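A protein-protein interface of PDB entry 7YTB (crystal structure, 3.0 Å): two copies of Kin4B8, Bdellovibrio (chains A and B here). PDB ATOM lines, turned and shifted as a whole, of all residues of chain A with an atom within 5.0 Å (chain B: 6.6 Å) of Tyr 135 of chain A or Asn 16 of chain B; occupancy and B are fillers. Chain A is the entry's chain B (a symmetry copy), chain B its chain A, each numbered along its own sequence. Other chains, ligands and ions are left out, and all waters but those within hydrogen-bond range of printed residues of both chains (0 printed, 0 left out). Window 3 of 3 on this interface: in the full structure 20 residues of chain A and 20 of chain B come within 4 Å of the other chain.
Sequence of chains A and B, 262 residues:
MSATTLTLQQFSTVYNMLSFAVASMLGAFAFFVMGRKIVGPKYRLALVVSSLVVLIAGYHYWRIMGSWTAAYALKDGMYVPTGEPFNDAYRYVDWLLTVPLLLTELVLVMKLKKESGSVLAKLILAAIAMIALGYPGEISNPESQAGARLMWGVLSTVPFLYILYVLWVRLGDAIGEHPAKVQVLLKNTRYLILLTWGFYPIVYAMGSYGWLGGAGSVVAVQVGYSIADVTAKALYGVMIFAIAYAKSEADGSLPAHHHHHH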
ATOM      1  N   ALA A  89      17.538   0.091  -6.344  1.00  0.00           N
ATOM      2  CA  ALA A  89      18.441   1.002  -5.656  1.00  0.00           C
ATOM      3  C   ALA A  89      18.880   0.483  -4.296  1.00  0.00           C
ATOM      4  O   ALA A  89      19.848   1.009  -3.735  1.00  0.00           O
ATOM      5  CB  ALA A  89      17.779   2.372  -5.500  1.00  0.00           C
ATOM      6  N   TYR A  90      18.202  -0.529  -3.751  1.00  0.00           N
ATOM      7  CA  TYR A  90      18.741  -1.184  -2.564  1.00  0.00           C
ATOM      8  C   TYR A  90      20.000  -1.970  -2.899  1.00  0.00           C
ATOM      9  O   TYR A  90      20.850  -2.187  -2.029  1.00  0.00           O
ATOM     10  CB  TYR A  90      17.711  -2.104  -1.918  1.00  0.00           C
ATOM     11  CG  TYR A  90      18.185  -2.571  -0.563  1.00  0.00           C
ATOM     12  CD1 TYR A  90      18.221  -1.706   0.521  1.00  0.00           C
ATOM     13  CD2 TYR A  90      18.664  -3.863  -0.389  1.00  0.00           C
ATOM     14  CE1 TYR A  90      18.681  -2.127   1.753  1.00  0.00           C
ATOM     15  CE2 TYR A  90      19.128  -4.293   0.838  1.00  0.00           C
ATOM     16  CZ  TYR A  90      19.135  -3.422   1.907  1.00  0.00           C
ATOM     17  OH  TYR A  90      19.596  -3.851   3.131  1.00  0.00           O
ATOM     18  N   TYR A  92      22.403  -0.972  -4.857  1.00  0.00           N
ATOM     19  CA  TYR A  92      23.562  -0.088  -4.894  1.00  0.00           C
ATOM     20  C   TYR A  92      24.202   0.034  -3.518  1.00  0.00           C
ATOM     21  O   TYR A  92      25.419   0.217  -3.412  1.00  0.00           O
ATOM     22  CB  TYR A  92      23.159   1.291  -5.408  1.00  0.00           C
ATOM     23  CG  TYR A  92      22.886   1.354  -6.893  1.00  0.00           C
ATOM     24  CD1 TYR A  92      21.890   0.580  -7.472  1.00  0.00           C
ATOM     25  CD2 TYR A  92      23.620   2.199  -7.714  1.00  0.00           C
ATOM     26  CE1 TYR A  92      21.634   0.641  -8.830  1.00  0.00           C
ATOM     27  CE2 TYR A  92      23.371   2.266  -9.072  1.00  0.00           C
ATOM     28  CZ  TYR A  92      22.377   1.485  -9.625  1.00  0.00           C
ATOM     29  OH  TYR A  92      22.124   1.546 -10.978  1.00  0.00           O
ATOM     30  N   VAL A  93      23.398  -0.058  -2.457  1.00  0.00           N
ATOM     31  CA  VAL A  93      23.934  -0.041  -1.100  1.00  0.00           C
ATOM     32  C   VAL A  93      24.793  -1.272  -0.846  1.00  0.00           C
ATOM     33  O   VAL A  93      25.792  -1.206  -0.117  1.00  0.00           O
ATOM     34  CB  VAL A  93      22.769   0.055  -0.093  1.00  0.00           C
ATOM     35  CG1 VAL A  93      23.247  -0.196   1.323  1.00  0.00           C
ATOM     36  CG2 VAL A  93      22.107   1.408  -0.200  1.00  0.00           C
ATOM     37  N   ILE A 131      29.836   3.512  -8.556  1.00  0.00           N
ATOM     38  CA  ILE A 131      28.538   3.340  -7.908  1.00  0.00           C
ATOM     39  C   ILE A 131      27.937   4.692  -7.549  1.00  0.00           C
ATOM     40  O   ILE A 131      26.727   4.909  -7.688  1.00  0.00           O
ATOM     41  CB  ILE A 131      28.672   2.434  -6.671  1.00  0.00           C
ATOM     42  CG1 ILE A 131      29.391   1.132  -7.034  1.00  0.00           C
ATOM     43  CG2 ILE A 131      27.305   2.151  -6.071  1.00  0.00           C
ATOM     44  CD1 ILE A 131      28.606   0.230  -7.965  1.00  0.00           C
ATOM     45  N   ALA A 132      28.771   5.619  -7.070  1.00  0.00           N
ATOM     46  CA  ALA A 132      28.277   6.928  -6.654  1.00  0.00           C
ATOM     47  C   ALA A 132      27.669   7.688  -7.826  1.00  0.00           C
ATOM     48  O   ALA A 132      26.592   8.278  -7.701  1.00  0.00           O
ATOM     49  CB  ALA A 132      29.401   7.740  -6.012  1.00  0.00           C
ATOM     50  N   LEU A 133      28.354   7.707  -8.970  1.00  0.00           N
ATOM     51  CA  LEU A 133      27.794   8.372 -10.144  1.00  0.00           C
ATOM     52  C   LEU A 133      26.593   7.616 -10.702  1.00  0.00           C
ATOM     53  O   LEU A 133      25.689   8.231 -11.277  1.00  0.00           O
ATOM     54  CB  LEU A 133      28.870   8.547 -11.220  1.00  0.00           C
ATOM     55  CG  LEU A 133      30.072   9.417 -10.845  1.00  0.00           C
ATOM     56  CD1 LEU A 133      31.089   9.480 -11.978  1.00  0.00           C
ATOM     57  CD2 LEU A 133      29.618  10.816 -10.458  1.00  0.00           C
ATOM     58  N   GLY A 134      26.575   6.289 -10.561  1.00  0.00           N
ATOM     59  CA  GLY A 134      25.451   5.512 -11.052  1.00  0.00           C
ATOM     60  C   GLY A 134      24.161   5.758 -10.295  1.00  0.00           C
ATOM     61  O   GLY A 134      23.072   5.621 -10.862  1.00  0.00           O
ATOM     62  N   TYR A 135      24.260   6.111  -9.005  1.00  0.00           N
ATOM     63  CA  TYR A 135      23.060   6.221  -8.179  1.00  0.00           C
ATOM     64  C   TYR A 135      22.118   7.342  -8.626  1.00  0.00           C
ATOM     65  O   TYR A 135      20.912   7.077  -8.762  1.00  0.00           O
ATOM     66  CB  TYR A 135      23.445   6.350  -6.700  1.00  0.00           C
ATOM     67  CG  TYR A 135      22.271   6.207  -5.757  1.00  0.00           C
ATOM     68  CD1 TYR A 135      21.824   4.954  -5.358  1.00  0.00           C
ATOM     69  CD2 TYR A 135      21.604   7.323  -5.274  1.00  0.00           C
ATOM     70  CE1 TYR A 135      20.746   4.820  -4.498  1.00  0.00           C
ATOM     71  CE2 TYR A 135      20.525   7.199  -4.413  1.00  0.00           C
ATOM     72  CZ  TYR A 135      20.101   5.945  -4.031  1.00  0.00           C
ATOM     73  OH  TYR A 135      19.027   5.818  -3.175  1.00  0.00           O
ATOM     74  N   PRO A 136      22.574   8.588  -8.847  1.00  0.00           N
ATOM     75  CA  PRO A 136      21.646   9.598  -9.397  1.00  0.00           C
ATOM     76  C   PRO A 136      20.949   9.156 -10.671  1.00  0.00           C
ATOM     77  O   PRO A 136      19.773   9.483 -10.873  1.00  0.00           O
ATOM     78  CB  PRO A 136      22.552  10.811  -9.646  1.00  0.00           C
ATOM     79  CG  PRO A 136      23.697  10.649  -8.743  1.00  0.00           C
ATOM     80  CD  PRO A 136      23.838   9.195  -8.399  1.00  0.00           C
ATOM     81  N   GLY A 137      21.643   8.424 -11.542  1.00  0.00           N
ATOM     82  CA  GLY A 137      21.017   7.979 -12.773  1.00  0.00           C
ATOM     83  C   GLY A 137      19.996   6.882 -12.561  1.00  0.00           C
ATOM     84  O   GLY A 137      19.010   6.798 -13.299  1.00  0.00           O
ATOM     85  N   GLU A 138      20.211   6.028 -11.557  1.00  0.00           N
ATOM     86  CA  GLU A 138      19.294   4.916 -11.326  1.00  0.00           C
ATOM     87  C   GLU A 138      17.950   5.400 -10.802  1.00  0.00           C
ATOM     88  O   GLU A 138      16.899   4.893 -11.212  1.00  0.00           O
ATOM     89  CB  GLU A 138      19.914   3.907 -10.360  1.00  0.00           C
ATOM     90  CG  GLU A 138      18.944   2.839  -9.859  1.00  0.00           C
ATOM     91  CD  GLU A 138      18.538   1.825 -10.923  1.00  0.00           C
ATOM     92  OE1 GLU A 138      18.943   1.963 -12.098  1.00  0.00           O
ATOM     93  OE2 GLU A 138      17.787   0.890 -10.582  1.00  0.00           O
ATOM     94  N   ILE A 139      17.958   6.387  -9.901  1.00  0.00           N
ATOM     95  CA  ILE A 139      16.712   6.877  -9.315  1.00  0.00           C
ATOM     96  C   ILE A 139      16.012   7.879 -10.213  1.00  0.00           C
ATOM     97  O   ILE A 139      14.911   8.334  -9.876  1.00  0.00           O
ATOM     98  CB  ILE A 139      16.959   7.517  -7.935  1.00  0.00           C
ATOM     99  CG1 ILE A 139      17.959   8.673  -8.048  1.00  0.00           C
ATOM    100  CG2 ILE A 139      17.442   6.470  -6.938  1.00  0.00           C
ATOM    101  CD1 ILE A 139      18.342   9.276  -6.713  1.00  0.00           C
ATOM    102  N   GLN B   9      11.552   9.226  -2.333  1.00  0.00           N
ATOM    103  CA  GLN B   9      13.006   9.261  -2.435  1.00  0.00           C
ATOM    104  C   GLN B   9      13.651   9.528  -1.081  1.00  0.00           C
ATOM    105  O   GLN B   9      14.640   8.883  -0.715  1.00  0.00           O
ATOM    106  CB  GLN B   9      13.424  10.323  -3.456  1.00  0.00           C
ATOM    107  CG  GLN B   9      14.919  10.566  -3.531  1.00  0.00           C
ATOM    108  CD  GLN B   9      15.300  11.460  -4.692  1.00  0.00           C
ATOM    109  OE1 GLN B   9      14.502  11.689  -5.603  1.00  0.00           O
ATOM    110  NE2 GLN B   9      16.524  11.975  -4.664  1.00  0.00           N
ATOM    111  N   PHE B  11      12.450   9.014   2.045  1.00  0.00           N
ATOM    112  CA  PHE B  11      12.332   7.856   2.926  1.00  0.00           C
ATOM    113  C   PHE B  11      13.264   6.732   2.487  1.00  0.00           C
ATOM    114  O   PHE B  11      13.884   6.066   3.325  1.00  0.00           O
ATOM    115  CB  PHE B  11      10.887   7.369   2.976  1.00  0.00           C
ATOM    116  CG  PHE B  11      10.667   6.214   3.915  1.00  0.00           C
ATOM    117  CD1 PHE B  11      10.502   6.428   5.275  1.00  0.00           C
ATOM    118  CD2 PHE B  11      10.607   4.916   3.434  1.00  0.00           C
ATOM    119  CE1 PHE B  11      10.289   5.370   6.138  1.00  0.00           C
ATOM    120  CE2 PHE B  11      10.394   3.855   4.291  1.00  0.00           C
ATOM    121  CZ  PHE B  11      10.235   4.082   5.644  1.00  0.00           C
ATOM    122  N   SER B  12      13.344   6.482   1.179  1.00  0.00           N
ATOM    123  CA  SER B  12      14.226   5.432   0.679  1.00  0.00           C
ATOM    124  C   SER B  12      15.689   5.749   0.967  1.00  0.00           C
ATOM    125  O   SER B  12      16.457   4.865   1.362  1.00  0.00           O
ATOM    126  CB  SER B  12      14.010   5.235  -0.821  1.00  0.00           C
ATOM    127  OG  SER B  12      12.662   4.894  -1.101  1.00  0.00           O
ATOM    128  N   THR B  13      16.094   7.006   0.760  1.00  0.00           N
ATOM    129  CA  THR B  13      17.489   7.396   0.964  1.00  0.00           C
ATOM    130  C   THR B  13      17.928   7.181   2.408  1.00  0.00           C
ATOM    131  O   THR B  13      18.985   6.595   2.663  1.00  0.00           O
ATOM    132  CB  THR B  13      17.691   8.857   0.560  1.00  0.00           C
ATOM    133  OG1 THR B  13      17.498   8.989  -0.854  1.00  0.00           O
ATOM    134  CG2 THR B  13      19.093   9.326   0.924  1.00  0.00           C
ATOM    135  N   VAL B  14      17.137   7.664   3.369  1.00  0.00           N
ATOM    136  CA  VAL B  14      17.511   7.504   4.772  1.00  0.00           C
ATOM    137  C   VAL B  14      17.506   6.031   5.154  1.00  0.00           C
ATOM    138  O   VAL B  14      18.384   5.565   5.888  1.00  0.00           O
ATOM    139  CB  VAL B  14      16.583   8.335   5.678  1.00  0.00           C
ATOM    140  CG1 VAL B  14      16.919   8.112   7.149  1.00  0.00           C
ATOM    141  CG2 VAL B  14      16.671   9.811   5.313  1.00  0.00           C
ATOM    142  N   TYR B  15      16.526   5.276   4.656  1.00  0.00           N
ATOM    143  CA  TYR B  15      16.483   3.842   4.925  1.00  0.00           C
ATOM    144  C   TYR B  15      17.715   3.138   4.372  1.00  0.00           C
ATOM    145  O   TYR B  15      18.261   2.229   5.009  1.00  0.00           O
ATOM    146  CB  TYR B  15      15.209   3.233   4.337  1.00  0.00           C
ATOM    147  CG  TYR B  15      15.159   1.724   4.430  1.00  0.00           C
ATOM    148  CD1 TYR B  15      14.695   1.089   5.574  1.00  0.00           C
ATOM    149  CD2 TYR B  15      15.560   0.932   3.362  1.00  0.00           C
ATOM    150  CE1 TYR B  15      14.647  -0.296   5.658  1.00  0.00           C
ATOM    151  CE2 TYR B  15      15.515  -0.450   3.436  1.00  0.00           C
ATOM    152  CZ  TYR B  15      15.057  -1.060   4.585  1.00  0.00           C
ATOM    153  OH  TYR B  15      15.009  -2.436   4.663  1.00  0.00           O
ATOM    154  N   ASN B  16      18.162   3.537   3.179  1.00  0.00           N
ATOM    155  CA  ASN B  16      19.318   2.887   2.572  1.00  0.00           C
ATOM    156  C   ASN B  16      20.595   3.178   3.355  1.00  0.00           C
ATOM    157  O   ASN B  16      21.402   2.271   3.594  1.00  0.00           O
ATOM    158  CB  ASN B  16      19.455   3.328   1.113  1.00  0.00           C
ATOM    159  CG  ASN B  16      18.327   2.811   0.238  1.00  0.00           C
ATOM    160  OD1 ASN B  16      17.508   2.000   0.673  1.00  0.00           O
ATOM    161  ND2 ASN B  16      18.286   3.273  -1.009  1.00  0.00           N
ATOM    162  N   MET B  17      20.792   4.435   3.770  1.00  0.00           N
ATOM    163  CA  MET B  17      21.962   4.794   4.569  1.00  0.00           C
ATOM    164  C   MET B  17      21.947   4.078   5.914  1.00  0.00           C
ATOM    165  O   MET B  17      23.005   3.768   6.472  1.00  0.00           O
ATOM    166  CB  MET B  17      21.996   6.316   4.752  1.00  0.00           C
ATOM    167  CG  MET B  17      23.344   6.984   5.055  1.00  0.00           C
ATOM    168  SD  MET B  17      24.843   6.252   4.370  1.00  0.00           S
ATOM    169  CE  MET B  17      25.449   5.355   5.794  1.00  0.00           C
ATOM    170  N   LEU B  18      20.756   3.782   6.439  1.00  0.00           N
ATOM    171  CA  LEU B  18      20.665   2.964   7.643  1.00  0.00           C
ATOM    172  C   LEU B  18      21.001   1.508   7.347  1.00  0.00           C
ATOM    173  O   LEU B  18      21.650   0.838   8.158  1.00  0.00           O
ATOM    174  CB  LEU B  18      19.268   3.084   8.246  1.00  0.00           C
ATOM    175  CG  LEU B  18      18.876   4.468   8.767  1.00  0.00           C
ATOM    176  CD1 LEU B  18      17.411   4.483   9.183  1.00  0.00           C
ATOM    177  CD2 LEU B  18      19.780   4.896   9.921  1.00  0.00           C
ATOM    178  N   SER B  19      20.564   1.000   6.192  1.00  0.00           N
ATOM    179  CA  SER B  19      20.919  -0.364   5.811  1.00  0.00           C
ATOM    180  C   SER B  19      22.393  -0.469   5.443  1.00  0.00           C
ATOM    181  O   SER B  19      23.026  -1.503   5.685  1.00  0.00           O
ATOM    182  CB  SER B  19      20.040  -0.832   4.648  1.00  0.00           C
ATOM    183  OG  SER B  19      19.077  -1.781   5.072  1.00  0.00           O
ATOM    184  N   PHE B  20      22.952   0.585   4.840  1.00  0.00           N
ATOM    185  CA  PHE B  20      24.392   0.635   4.618  1.00  0.00           C
ATOM    186  C   PHE B  20      25.146   0.548   5.941  1.00  0.00           C
ATOM    187  O   PHE B  20      26.142  -0.176   6.052  1.00  0.00           O
ATOM    188  CB  PHE B  20      24.769   1.911   3.863  1.00  0.00           C
ATOM    189  CG  PHE B  20      26.237   2.017   3.543  1.00  0.00           C
ATOM    190  CD1 PHE B  20      26.773   1.303   2.483  1.00  0.00           C
ATOM    191  CD2 PHE B  20      27.084   2.808   4.303  1.00  0.00           C
ATOM    192  CE1 PHE B  20      28.118   1.390   2.176  1.00  0.00           C
ATOM    193  CE2 PHE B  20      28.432   2.895   4.002  1.00  0.00           C
ATOM    194  CZ  PHE B  20      28.948   2.185   2.938  1.00  0.00           C
ATOM    195  N   ALA B  21      24.685   1.290   6.953  1.00  0.00           N
ATOM    196  CA  ALA B  21      25.356   1.281   8.250  1.00  0.00           C
ATOM    197  C   ALA B  21      25.299  -0.095   8.900  1.00  0.00           C
ATOM    198  O   ALA B  21      26.298  -0.569   9.452  1.00  0.00           O
ATOM    199  CB  ALA B  21      24.735   2.334   9.167  1.00  0.00           C
ATOM    200  N   TRP B  68      12.773   3.812  12.174  1.00  0.00           N
ATOM    201  CA  TRP B  68      12.557   4.667  11.011  1.00  0.00           C
ATOM    202  C   TRP B  68      11.392   4.166  10.168  1.00  0.00           C
ATOM    203  O   TRP B  68      10.509   4.944   9.788  1.00  0.00           O
ATOM    204  CB  TRP B  68      13.838   4.739  10.175  1.00  0.00           C
ATOM    205  CG  TRP B  68      13.672   5.510   8.906  1.00  0.00           C
ATOM    206  CD1 TRP B  68      13.534   4.993   7.652  1.00  0.00           C
ATOM    207  CD2 TRP B  68      13.643   6.937   8.756  1.00  0.00           C
ATOM    208  NE1 TRP B  68      13.412   6.005   6.732  1.00  0.00           N
ATOM    209  CE2 TRP B  68      13.477   7.208   7.383  1.00  0.00           C
ATOM    210  CE3 TRP B  68      13.739   8.010   9.648  1.00  0.00           C
ATOM    211  CZ2 TRP B  68      13.400   8.505   6.881  1.00  0.00           C
ATOM    212  CZ3 TRP B  68      13.667   9.299   9.146  1.00  0.00           C
ATOM    213  CH2 TRP B  68      13.502   9.534   7.775  1.00  0.00           C
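The side-chain hydroxyl of Tyr 135 of chain A is in hydrogen-bond range of the side-chain amide nitrogen of Asn 16 of chain B, 3.4 Å away.
The side-chain hydroxyl (OG) of Ser 19 of chain B is in hydrogen-bond range of the side-chain hydroxyl (OH) of Tyr 90 of chain A, at 2.9 Å.
Printed residues of chain A that touch a printed residue of chain B: Ala 89, Tyr 90, Val 93, Tyr 135 and Ile 139.
Of the 13 printed residues of chain B, 5 touch a printed residue of chain A.
Among the printed residues, 8 pairs touch across the chains.
Of the printed residues of chain B, Tyr 135 of chain A touches Asn 16.
Of chain A, only Ala 89, Tyr 90, Val 93 and Tyr 135 come within 4 Å of Asn 16 of chain B.
Of the printed residues of chain B, Ile 139 of chain A touches Gln 9 (3.8 Å).
Of the printed residues of chain B, Val 93 of chain A touches Asn 16 and Phe 20.
Printed residues of chain A within 4 Å of Gln 9 of chain B: Ile 139 (3.8 Å).
Printed residues of chain B within 4 Å of Tyr 90 of chain A: Tyr 15, Asn 16 and Ser 19.
Gly 134 of chain A touches none of the printed residues of chain B.
Leu 133 of chain A touches none of the printed residues of chain B.
The nearest printed residue of chain A that does not touch Asn 16 of chain B is Ile 139 of chain A (6.8 Å).
The nearest printed residue of chain A that does not touch Tyr 15 of chain B is Val 93 of chain A (6.5 Å).
Ala 89 of chain A touches Asn 16 of chain B (O to ND2, 3.9 Å).
Tyr 90 of chain A touches Tyr 15 of chain B (CE1 to CE2, 3.96 Å).
Asn 16 of chain B touches Tyr 90 of chain A (OD1 to CD1, 3.8 Å).
Asn 16 of chain B touches Val 93 of chain A (CB to CG2, 3.5 Å).
Val 93 of chain A touches Phe 20 of chain B.
Ile 139 of chain A touches Gln 9 of chain B.
No position is printed for both chains.
Of the 8 pairs that touch across the chains among the printed residues, none has its exchanged pair printed and touching as well.
OG1 of Thr 13 of chain B lies within hydrogen-bond range of O of Gln 9 of chain B.
The side-chain amide oxygen of Asn 16 of chain B sits close to the backbone carbonyl oxygen of Ser 12 of chain B (3.1 Å).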
